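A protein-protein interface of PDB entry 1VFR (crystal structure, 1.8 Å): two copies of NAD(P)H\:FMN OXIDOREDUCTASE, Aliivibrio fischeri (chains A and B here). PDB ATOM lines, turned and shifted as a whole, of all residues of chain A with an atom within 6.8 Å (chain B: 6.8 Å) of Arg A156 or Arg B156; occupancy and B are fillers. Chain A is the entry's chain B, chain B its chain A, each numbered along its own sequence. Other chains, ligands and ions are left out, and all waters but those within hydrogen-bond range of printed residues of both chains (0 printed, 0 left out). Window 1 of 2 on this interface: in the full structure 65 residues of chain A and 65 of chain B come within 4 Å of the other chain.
Hydrophobic or aromatic side chains of chain B within 4 Å of the printed part of chain A: Ile B5, His B152 and Leu B157. Among the printed residues, Asp or Glu carboxylates within 4 Å of a Lys or Arg side-chain nitrogen of the other chain: Asp A8 with Arg B156 (2.9 Å) and Arg A156 with Asp B8 (2.8 Å).
ND1 of His B3 lies within hydrogen-bond range of N of Ile B5, at 3.2 Å. A ring nitrogen (ND1) of His A3 sits at hydrogen-bond distance from the backbone NH of Ile A5 (3.2 Å).
Arg A156 touches just these residues of chain B: Pro B4 (3.9 Å), Ile B5 (3.6 Å), Asp B8 (2.8 Å), His B152 (3.0 Å) and Arg B156 (3.6 Å). Of chain A, only Pro A4 (3.9 Å), Ile A5 (3.7 Å), Asp A8 (2.9 Å), His A152 (3.0 Å) and Arg A156 (3.6 Å) come within 4 Å of Arg B156. Printed residues of chain A within 4 Å of His B152: His A152 (3.6 Å), Thr A153 (3.2 Å) and Arg A156 (3.0 Å). Of the printed residues of chain B, Pro A4 touches Arg B156 (3.9 Å). Printed residues of chain B within 4 Å of Leu A157: Ile B5 (3.7 Å). Ile A6 touches none of the printed residues of chain B. The nearest residue of chain A that does not touch Arg B156 is Leu A9 (5.9 Å). The nearest printed residue of chain B that does not touch His A152 is Ile B5 (6.0 Å).
O of Pro A4 touches NH2 of Arg B156, 3.9 Å away. Ile A5 touches Thr B153 (CD1 to O, 3.9 Å). Ile A5 touches Arg B156. Leu B157 touches Ile A5. His A152 touches His B152. Thr A153 touches His B152 (OG1 to CE1, 3.2 Å). NH2 of Arg A156 touches O of Pro B4, 3.9 Å away. Ile B5 touches Arg A156. Arg A156 touches Arg B156 (CG to NH1, 3.6 Å). CD1 of Ile B5 touches CG of Leu A157 (3.7 Å).
Pro A4 touches Arg B156, and with the chains exchanged Arg A156 touches Pro B4. Ile A5 touches Arg B156, and with the chains exchanged Arg A156 touches Ile B5. Asp A8 touches Arg B156, and with the chains exchanged Arg A156 touches Asp B8. His A152 touches Arg B156, and with the chains exchanged Arg A156 touches His B152. 15 positions are printed for both chains.
The guanidinium group of Arg B156 lies within salt-bridge range of the side-chain carboxylate of Asp A8, at 2.9 Å. NH1 of Arg B156 lies within hydrogen-bond range of NE2 of His A152. The guanidinium group (NH1) of Arg A156 sits at hydrogen-bond distance from a ring nitrogen (NE2) of His B152. OD2 of Asp B8 is in salt-bridge range of NH1 of Arg A156, 2.8 Å away.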
ATOM      1  N   HIS A   3     -14.432 -10.553 -25.226  1.00  0.00           N
ATOM      2  CA  HIS A   3     -14.816 -11.743 -24.485  1.00  0.00           C
ATOM      3  C   HIS A   3     -13.770 -12.799 -24.860  1.00  0.00           C
ATOM      4  O   HIS A   3     -13.436 -12.938 -26.031  1.00  0.00           O
ATOM      5  CB  HIS A   3     -16.198 -12.185 -24.946  1.00  0.00           C
ATOM      6  CG  HIS A   3     -16.798 -13.260 -24.103  1.00  0.00           C
ATOM      7  ND1 HIS A   3     -16.331 -14.556 -24.103  1.00  0.00           N
ATOM      8  CD2 HIS A   3     -17.854 -13.239 -23.254  1.00  0.00           C
ATOM      9  CE1 HIS A   3     -17.077 -15.287 -23.295  1.00  0.00           C
ATOM     10  NE2 HIS A   3     -18.011 -14.511 -22.770  1.00  0.00           N
ATOM     11  N   PRO A   4     -13.236 -13.543 -23.873  1.00  0.00           N
ATOM     12  CA  PRO A   4     -12.214 -14.576 -24.127  1.00  0.00           C
ATOM     13  C   PRO A   4     -12.558 -15.584 -25.240  1.00  0.00           C
ATOM     14  O   PRO A   4     -11.718 -15.887 -26.076  1.00  0.00           O
ATOM     15  CB  PRO A   4     -12.067 -15.253 -22.764  1.00  0.00           C
ATOM     16  CG  PRO A   4     -12.363 -14.158 -21.808  1.00  0.00           C
ATOM     17  CD  PRO A   4     -13.535 -13.445 -22.433  1.00  0.00           C
ATOM     18  N   ILE A   5     -13.798 -16.062 -25.268  1.00  0.00           N
ATOM     19  CA  ILE A   5     -14.210 -17.020 -26.284  1.00  0.00           C
ATOM     20  C   ILE A   5     -14.197 -16.416 -27.682  1.00  0.00           C
ATOM     21  O   ILE A   5     -13.666 -17.009 -28.636  1.00  0.00           O
ATOM     22  CB  ILE A   5     -15.582 -17.608 -25.973  1.00  0.00           C
ATOM     23  CG1 ILE A   5     -15.533 -18.324 -24.621  1.00  0.00           C
ATOM     24  CG2 ILE A   5     -15.982 -18.602 -27.075  1.00  0.00           C
ATOM     25  CD1 ILE A   5     -16.839 -18.931 -24.194  1.00  0.00           C
ATOM     26  N   ILE A   6     -14.740 -15.209 -27.797  1.00  0.00           N
ATOM     27  CA  ILE A   6     -14.789 -14.529 -29.080  1.00  0.00           C
ATOM     28  C   ILE A   6     -13.393 -14.168 -29.574  1.00  0.00           C
ATOM     29  O   ILE A   6     -13.098 -14.282 -30.760  1.00  0.00           O
ATOM     30  CB  ILE A   6     -15.693 -13.271 -29.019  1.00  0.00           C
ATOM     31  CG1 ILE A   6     -17.117 -13.673 -28.645  1.00  0.00           C
ATOM     32  CG2 ILE A   6     -15.687 -12.554 -30.353  1.00  0.00           C
ATOM     33  CD1 ILE A   6     -17.711 -14.759 -29.562  1.00  0.00           C
ATOM     34  N   ASP A   8     -10.607 -15.767 -29.013  1.00  0.00           N
ATOM     35  CA  ASP A   8      -9.980 -16.996 -29.509  1.00  0.00           C
ATOM     36  C   ASP A   8     -10.483 -17.368 -30.895  1.00  0.00           C
ATOM     37  O   ASP A   8      -9.685 -17.672 -31.764  1.00  0.00           O
ATOM     38  CB  ASP A   8     -10.263 -18.170 -28.571  1.00  0.00           C
ATOM     39  CG  ASP A   8      -9.470 -18.101 -27.279  1.00  0.00           C
ATOM     40  OD1 ASP A   8      -8.574 -17.262 -27.145  1.00  0.00           O
ATOM     41  OD2 ASP A   8      -9.767 -18.879 -26.371  1.00  0.00           O
ATOM     42  N   LEU A   9     -11.797 -17.284 -31.104  1.00  0.00           N
ATOM     43  CA  LEU A   9     -12.399 -17.646 -32.391  1.00  0.00           C
ATOM     44  C   LEU A   9     -12.199 -16.619 -33.498  1.00  0.00           C
ATOM     45  O   LEU A   9     -12.232 -16.955 -34.674  1.00  0.00           O
ATOM     46  CB  LEU A   9     -13.870 -18.010 -32.209  1.00  0.00           C
ATOM     47  CG  LEU A   9     -14.046 -19.231 -31.299  1.00  0.00           C
ATOM     48  CD1 LEU A   9     -15.512 -19.515 -31.095  1.00  0.00           C
ATOM     49  CD2 LEU A   9     -13.343 -20.457 -31.887  1.00  0.00           C
ATOM     50  N   LEU A 151     -10.068 -27.712 -33.291  1.00  0.00           N
ATOM     51  CA  LEU A 151      -9.798 -26.362 -33.740  1.00  0.00           C
ATOM     52  C   LEU A 151     -10.001 -25.354 -32.617  1.00  0.00           C
ATOM     53  O   LEU A 151      -9.234 -24.403 -32.490  1.00  0.00           O
ATOM     54  CB  LEU A 151     -10.658 -26.028 -34.954  1.00  0.00           C
ATOM     55  CG  LEU A 151     -10.288 -26.764 -36.245  1.00  0.00           C
ATOM     56  CD1 LEU A 151     -11.348 -26.441 -37.313  1.00  0.00           C
ATOM     57  CD2 LEU A 151      -8.906 -26.338 -36.722  1.00  0.00           C
ATOM     58  N   HIS A 152     -10.987 -25.595 -31.767  1.00  0.00           N
ATOM     59  CA  HIS A 152     -11.238 -24.694 -30.646  1.00  0.00           C
ATOM     60  C   HIS A 152     -10.097 -24.883 -29.639  1.00  0.00           C
ATOM     61  O   HIS A 152      -9.570 -23.923 -29.105  1.00  0.00           O
ATOM     62  CB  HIS A 152     -12.600 -24.998 -29.999  1.00  0.00           C
ATOM     63  CG  HIS A 152     -13.119 -23.891 -29.121  1.00  0.00           C
ATOM     64  ND1 HIS A 152     -14.407 -23.401 -29.219  1.00  0.00           N
ATOM     65  CD2 HIS A 152     -12.532 -23.194 -28.115  1.00  0.00           C
ATOM     66  CE1 HIS A 152     -14.593 -22.456 -28.313  1.00  0.00           C
ATOM     67  NE2 HIS A 152     -13.472 -22.310 -27.629  1.00  0.00           N
ATOM     68  N   THR A 153      -9.706 -26.131 -29.409  1.00  0.00           N
ATOM     69  CA  THR A 153      -8.615 -26.447 -28.490  1.00  0.00           C
ATOM     70  C   THR A 153      -7.300 -25.759 -28.916  1.00  0.00           C
ATOM     71  O   THR A 153      -6.599 -25.171 -28.077  1.00  0.00           O
ATOM     72  CB  THR A 153      -8.414 -27.962 -28.388  1.00  0.00           C
ATOM     73  OG1 THR A 153      -9.565 -28.559 -27.777  1.00  0.00           O
ATOM     74  CG2 THR A 153      -7.168 -28.277 -27.536  1.00  0.00           C
ATOM     75  N   LEU A 154      -6.981 -25.808 -30.212  1.00  0.00           N
ATOM     76  CA  LEU A 154      -5.768 -25.172 -30.749  1.00  0.00           C
ATOM     77  C   LEU A 154      -5.795 -23.642 -30.614  1.00  0.00           C
ATOM     78  O   LEU A 154      -4.760 -23.001 -30.417  1.00  0.00           O
ATOM     79  CB  LEU A 154      -5.541 -25.567 -32.214  1.00  0.00           C
ATOM     80  CG  LEU A 154      -5.164 -27.039 -32.443  1.00  0.00           C
ATOM     81  CD1 LEU A 154      -5.423 -27.445 -33.896  1.00  0.00           C
ATOM     82  CD2 LEU A 154      -3.705 -27.262 -32.080  1.00  0.00           C
ATOM     83  N   ALA A 155      -6.982 -23.055 -30.720  1.00  0.00           N
ATOM     84  CA  ALA A 155      -7.123 -21.614 -30.576  1.00  0.00           C
ATOM     85  C   ALA A 155      -6.754 -21.195 -29.135  1.00  0.00           C
ATOM     86  O   ALA A 155      -6.107 -20.166 -28.928  1.00  0.00           O
ATOM     87  CB  ALA A 155      -8.556 -21.189 -30.923  1.00  0.00           C
ATOM     88  N   ARG A 156      -7.126 -22.022 -28.159  1.00  0.00           N
ATOM     89  CA  ARG A 156      -6.829 -21.774 -26.748  1.00  0.00           C
ATOM     90  C   ARG A 156      -5.345 -21.979 -26.413  1.00  0.00           C
ATOM     91  O   ARG A 156      -4.830 -21.351 -25.495  1.00  0.00           O
ATOM     92  CB  ARG A 156      -7.693 -22.664 -25.848  1.00  0.00           C
ATOM     93  CG  ARG A 156      -9.182 -22.412 -26.007  1.00  0.00           C
ATOM     94  CD  ARG A 156      -9.996 -23.288 -25.104  1.00  0.00           C
ATOM     95  NE  ARG A 156      -9.830 -22.940 -23.703  1.00  0.00           N
ATOM     96  CZ  ARG A 156     -10.464 -23.549 -22.707  1.00  0.00           C
ATOM     97  NH1 ARG A 156     -11.312 -24.539 -22.943  1.00  0.00           N
ATOM     98  NH2 ARG A 156     -10.254 -23.167 -21.458  1.00  0.00           N
ATOM     99  N   LEU A 157      -4.668 -22.861 -27.148  1.00  0.00           N
ATOM    100  CA  LEU A 157      -3.245 -23.127 -26.917  1.00  0.00           C
ATOM    101  C   LEU A 157      -2.343 -22.192 -27.717  1.00  0.00           C
ATOM    102  O   LEU A 157      -1.127 -22.172 -27.518  1.00  0.00           O
ATOM    103  CB  LEU A 157      -2.928 -24.570 -27.301  1.00  0.00           C
ATOM    104  CG  LEU A 157      -3.451 -25.666 -26.372  1.00  0.00           C
ATOM    105  CD1 LEU A 157      -3.225 -27.033 -27.021  1.00  0.00           C
ATOM    106  CD2 LEU A 157      -2.741 -25.557 -25.024  1.00  0.00           C
ATOM    107  N   ASN A 158      -2.949 -21.390 -28.590  1.00  0.00           N
ATOM    108  CA  ASN A 158      -2.220 -20.466 -29.462  1.00  0.00           C
ATOM    109  C   ASN A 158      -1.230 -21.166 -30.393  1.00  0.00           C
ATOM    110  O   ASN A 158      -0.072 -20.760 -30.543  1.00  0.00           O
ATOM    111  CB  ASN A 158      -1.546 -19.366 -28.647  1.00  0.00           C
ATOM    112  CG  ASN A 158      -2.537 -18.296 -28.208  1.00  0.00           C
ATOM    113  OD1 ASN A 158      -2.873 -17.412 -28.980  1.00  0.00           O
ATOM    114  ND2 ASN A 158      -3.019 -18.389 -26.977  1.00  0.00           N
ATOM    115  N   ILE A 159      -1.726 -22.227 -31.018  1.00  0.00           N
ATOM    116  CA  ILE A 159      -0.967 -23.029 -31.961  1.00  0.00           C
ATOM    117  C   ILE A 159      -1.671 -22.856 -33.296  1.00  0.00           C
ATOM    118  O   ILE A 159      -2.903 -22.880 -33.349  1.00  0.00           O
ATOM    119  CB  ILE A 159      -0.976 -24.520 -31.540  1.00  0.00           C
ATOM    120  CG1 ILE A 159      -0.165 -24.699 -30.251  1.00  0.00           C
ATOM    121  CG2 ILE A 159      -0.438 -25.399 -32.657  1.00  0.00           C
ATOM    122  CD1 ILE A 159      -0.308 -26.076 -29.626  1.00  0.00           C
ATOM    123  N   HIS B   3      -5.275 -28.590 -16.018  1.00  0.00           N
ATOM    124  CA  HIS B   3      -5.092 -27.709 -17.158  1.00  0.00           C
ATOM    125  C   HIS B   3      -6.503 -27.192 -17.502  1.00  0.00           C
ATOM    126  O   HIS B   3      -7.444 -27.979 -17.558  1.00  0.00           O
ATOM    127  CB  HIS B   3      -4.504 -28.516 -18.318  1.00  0.00           C
ATOM    128  CG  HIS B   3      -4.062 -27.676 -19.475  1.00  0.00           C
ATOM    129  ND1 HIS B   3      -4.947 -27.011 -20.299  1.00  0.00           N
ATOM    130  CD2 HIS B   3      -2.828 -27.395 -19.947  1.00  0.00           C
ATOM    131  CE1 HIS B   3      -4.276 -26.355 -21.226  1.00  0.00           C
ATOM    132  NE2 HIS B   3      -2.988 -26.573 -21.036  1.00  0.00           N
ATOM    133  N   PRO B   4      -6.664 -25.872 -17.717  1.00  0.00           N
ATOM    134  CA  PRO B   4      -7.986 -25.289 -18.039  1.00  0.00           C
ATOM    135  C   PRO B   4      -8.755 -26.005 -19.165  1.00  0.00           C
ATOM    136  O   PRO B   4      -9.954 -26.239 -19.043  1.00  0.00           O
ATOM    137  CB  PRO B   4      -7.647 -23.841 -18.428  1.00  0.00           C
ATOM    138  CG  PRO B   4      -6.400 -23.563 -17.649  1.00  0.00           C
ATOM    139  CD  PRO B   4      -5.611 -24.842 -17.744  1.00  0.00           C
ATOM    140  N   ILE B   5      -8.075 -26.348 -20.252  1.00  0.00           N
ATOM    141  CA  ILE B   5      -8.739 -27.024 -21.376  1.00  0.00           C
ATOM    142  C   ILE B   5      -9.245 -28.405 -20.976  1.00  0.00           C
ATOM    143  O   ILE B   5     -10.402 -28.762 -21.248  1.00  0.00           O
ATOM    144  CB  ILE B   5      -7.816 -27.124 -22.602  1.00  0.00           C
ATOM    145  CG1 ILE B   5      -7.407 -25.715 -23.044  1.00  0.00           C
ATOM    146  CG2 ILE B   5      -8.516 -27.851 -23.750  1.00  0.00           C
ATOM    147  CD1 ILE B   5      -6.482 -25.666 -24.231  1.00  0.00           C
ATOM    148  N   ILE B   6      -8.402 -29.163 -20.275  1.00  0.00           N
ATOM    149  CA  ILE B   6      -8.780 -30.501 -19.835  1.00  0.00           C
ATOM    150  C   ILE B   6      -9.906 -30.463 -18.812  1.00  0.00           C
ATOM    151  O   ILE B   6     -10.819 -31.285 -18.861  1.00  0.00           O
ATOM    152  CB  ILE B   6      -7.558 -31.271 -19.271  1.00  0.00           C
ATOM    153  CG1 ILE B   6      -6.493 -31.404 -20.358  1.00  0.00           C
ATOM    154  CG2 ILE B   6      -7.973 -32.633 -18.738  1.00  0.00           C
ATOM    155  CD1 ILE B   6      -6.996 -31.996 -21.657  1.00  0.00           C
ATOM    156  N   ASP B   8     -12.308 -28.276 -18.584  1.00  0.00           N
ATOM    157  CA  ASP B   8     -13.551 -27.987 -19.298  1.00  0.00           C
ATOM    158  C   ASP B   8     -14.108 -29.220 -19.990  1.00  0.00           C
ATOM    159  O   ASP B   8     -15.300 -29.500 -19.903  1.00  0.00           O
ATOM    160  CB  ASP B   8     -13.335 -26.903 -20.356  1.00  0.00           C
ATOM    161  CG  ASP B   8     -13.163 -25.528 -19.762  1.00  0.00           C
ATOM    162  OD1 ASP B   8     -13.399 -25.365 -18.550  1.00  0.00           O
ATOM    163  OD2 ASP B   8     -12.786 -24.610 -20.518  1.00  0.00           O
ATOM    164  N   LEU B   9     -13.236 -29.970 -20.650  1.00  0.00           N
ATOM    165  CA  LEU B   9     -13.650 -31.151 -21.387  1.00  0.00           C
ATOM    166  C   LEU B   9     -13.971 -32.360 -20.509  1.00  0.00           C
ATOM    167  O   LEU B   9     -14.754 -33.231 -20.900  1.00  0.00           O
ATOM    168  CB  LEU B   9     -12.622 -31.474 -22.472  1.00  0.00           C
ATOM    169  CG  LEU B   9     -12.534 -30.371 -23.533  1.00  0.00           C
ATOM    170  CD1 LEU B   9     -11.453 -30.716 -24.529  1.00  0.00           C
ATOM    171  CD2 LEU B   9     -13.866 -30.203 -24.249  1.00  0.00           C
ATOM    172  N   LEU B 151     -20.038 -27.355 -28.575  1.00  0.00           N
ATOM    173  CA  LEU B 151     -19.914 -28.096 -27.336  1.00  0.00           C
ATOM    174  C   LEU B 151     -18.727 -27.594 -26.513  1.00  0.00           C
ATOM    175  O   LEU B 151     -18.806 -27.499 -25.294  1.00  0.00           O
ATOM    176  CB  LEU B 151     -19.805 -29.587 -27.624  1.00  0.00           C
ATOM    177  CG  LEU B 151     -21.100 -30.243 -28.120  1.00  0.00           C
ATOM    178  CD1 LEU B 151     -20.783 -31.678 -28.496  1.00  0.00           C
ATOM    179  CD2 LEU B 151     -22.208 -30.193 -27.048  1.00  0.00           C
ATOM    180  N   HIS B 152     -17.647 -27.225 -27.184  1.00  0.00           N
ATOM    181  CA  HIS B 152     -16.477 -26.703 -26.478  1.00  0.00           C
ATOM    182  C   HIS B 152     -16.835 -25.303 -25.926  1.00  0.00           C
ATOM    183  O   HIS B 152     -16.494 -24.975 -24.796  1.00  0.00           O
ATOM    184  CB  HIS B 152     -15.258 -26.629 -27.422  1.00  0.00           C
ATOM    185  CG  HIS B 152     -13.944 -26.509 -26.699  1.00  0.00           C
ATOM    186  ND1 HIS B 152     -12.855 -27.301 -26.998  1.00  0.00           N
ATOM    187  CD2 HIS B 152     -13.536 -25.674 -25.714  1.00  0.00           C
ATOM    188  CE1 HIS B 152     -11.831 -26.955 -26.237  1.00  0.00           C
ATOM    189  NE2 HIS B 152     -12.218 -25.970 -25.448  1.00  0.00           N
ATOM    190  N   THR B 153     -17.550 -24.505 -26.716  1.00  0.00           N
ATOM    191  CA  THR B 153     -17.952 -23.159 -26.306  1.00  0.00           C
ATOM    192  C   THR B 153     -18.849 -23.200 -25.067  1.00  0.00           C
ATOM    193  O   THR B 153     -18.663 -22.416 -24.133  1.00  0.00           O
ATOM    194  CB  THR B 153     -18.676 -22.426 -27.452  1.00  0.00           C
ATOM    195  OG1 THR B 153     -17.767 -22.191 -28.533  1.00  0.00           O
ATOM    196  CG2 THR B 153     -19.201 -21.096 -26.970  1.00  0.00           C
ATOM    197  N   LEU B 154     -19.790 -24.137 -25.041  1.00  0.00           N
ATOM    198  CA  LEU B 154     -20.698 -24.297 -23.914  1.00  0.00           C
ATOM    199  C   LEU B 154     -19.986 -24.728 -22.642  1.00  0.00           C
ATOM    200  O   LEU B 154     -20.381 -24.337 -21.541  1.00  0.00           O
ATOM    201  CB  LEU B 154     -21.799 -25.301 -24.241  1.00  0.00           C
ATOM    202  CG  LEU B 154     -22.829 -24.799 -25.266  1.00  0.00           C
ATOM    203  CD1 LEU B 154     -23.596 -25.982 -25.863  1.00  0.00           C
ATOM    204  CD2 LEU B 154     -23.775 -23.795 -24.615  1.00  0.00           C
ATOM    205  N   ALA B 155     -18.937 -25.537 -22.794  1.00  0.00           N
ATOM    206  CA  ALA B 155     -18.137 -25.984 -21.646  1.00  0.00           C
ATOM    207  C   ALA B 155     -17.454 -24.773 -21.000  1.00  0.00           C
ATOM    208  O   ALA B 155     -17.398 -24.675 -19.769  1.00  0.00           O
ATOM    209  CB  ALA B 155     -17.092 -27.027 -22.101  1.00  0.00           C
ATOM    210  N   ARG B 156     -16.980 -23.833 -21.821  1.00  0.00           N
ATOM    211  CA  ARG B 156     -16.320 -22.617 -21.334  1.00  0.00           C
ATOM    212  C   ARG B 156     -17.297 -21.651 -20.651  1.00  0.00           C
ATOM    213  O   ARG B 156     -16.918 -20.910 -19.755  1.00  0.00           O
ATOM    214  CB  ARG B 156     -15.591 -21.908 -22.481  1.00  0.00           C
ATOM    215  CG  ARG B 156     -14.481 -22.758 -23.105  1.00  0.00           C
ATOM    216  CD  ARG B 156     -13.771 -22.039 -24.209  1.00  0.00           C
ATOM    217  NE  ARG B 156     -12.997 -20.919 -23.699  1.00  0.00           N
ATOM    218  CZ  ARG B 156     -12.246 -20.139 -24.464  1.00  0.00           C
ATOM    219  NH1 ARG B 156     -12.161 -20.361 -25.771  1.00  0.00           N
ATOM    220  NH2 ARG B 156     -11.587 -19.118 -23.933  1.00  0.00           N
ATOM    221  N   LEU B 157     -18.549 -21.655 -21.095  1.00  0.00           N
ATOM    222  CA  LEU B 157     -19.597 -20.795 -20.531  1.00  0.00           C
ATOM    223  C   LEU B 157     -20.305 -21.427 -19.334  1.00  0.00           C
ATOM    224  O   LEU B 157     -21.126 -20.777 -18.658  1.00  0.00           O
ATOM    225  CB  LEU B 157     -20.644 -20.469 -21.612  1.00  0.00           C
ATOM    226  CG  LEU B 157     -20.219 -19.506 -22.727  1.00  0.00           C
ATOM    227  CD1 LEU B 157     -21.302 -19.441 -23.799  1.00  0.00           C
ATOM    228  CD2 LEU B 157     -19.940 -18.134 -22.129  1.00  0.00           C
ATOM    229  N   ASN B 158     -19.984 -22.684 -19.060  1.00  0.00           N
ATOM    230  CA  ASN B 158     -20.592 -23.424 -17.955  1.00  0.00           C
ATOM    231  C   ASN B 158     -22.109 -23.527 -18.064  1.00  0.00           C
ATOM    232  O   ASN B 158     -22.857 -23.300 -17.108  1.00  0.00           O
ATOM    233  CB  ASN B 158     -20.141 -22.854 -16.593  1.00  0.00           C
ATOM    234  CG  ASN B 158     -18.730 -23.291 -16.243  1.00  0.00           C
ATOM    235  OD1 ASN B 158     -18.526 -24.403 -15.773  1.00  0.00           O
ATOM    236  ND2 ASN B 158     -17.755 -22.446 -16.526  1.00  0.00           N
ATOM    237  N   ILE B 159     -22.542 -23.875 -19.265  1.00  0.00           N
ATOM    238  CA  ILE B 159     -23.944 -24.048 -19.583  1.00  0.00           C
ATOM    239  C   ILE B 159     -24.087 -25.526 -19.937  1.00  0.00           C
ATOM    240  O   ILE B 159     -23.250 -26.080 -20.631  1.00  0.00           O
ATOM    241  CB  ILE B 159     -24.344 -23.162 -20.790  1.00  0.00           C
ATOM    242  CG1 ILE B 159     -24.325 -21.687 -20.398  1.00  0.00           C
ATOM    243  CG2 ILE B 159     -25.720 -23.554 -21.309  1.00  0.00           C
ATOM    244  CD1 ILE B 159     -24.410 -20.760 -21.587  1.00  0.00           C
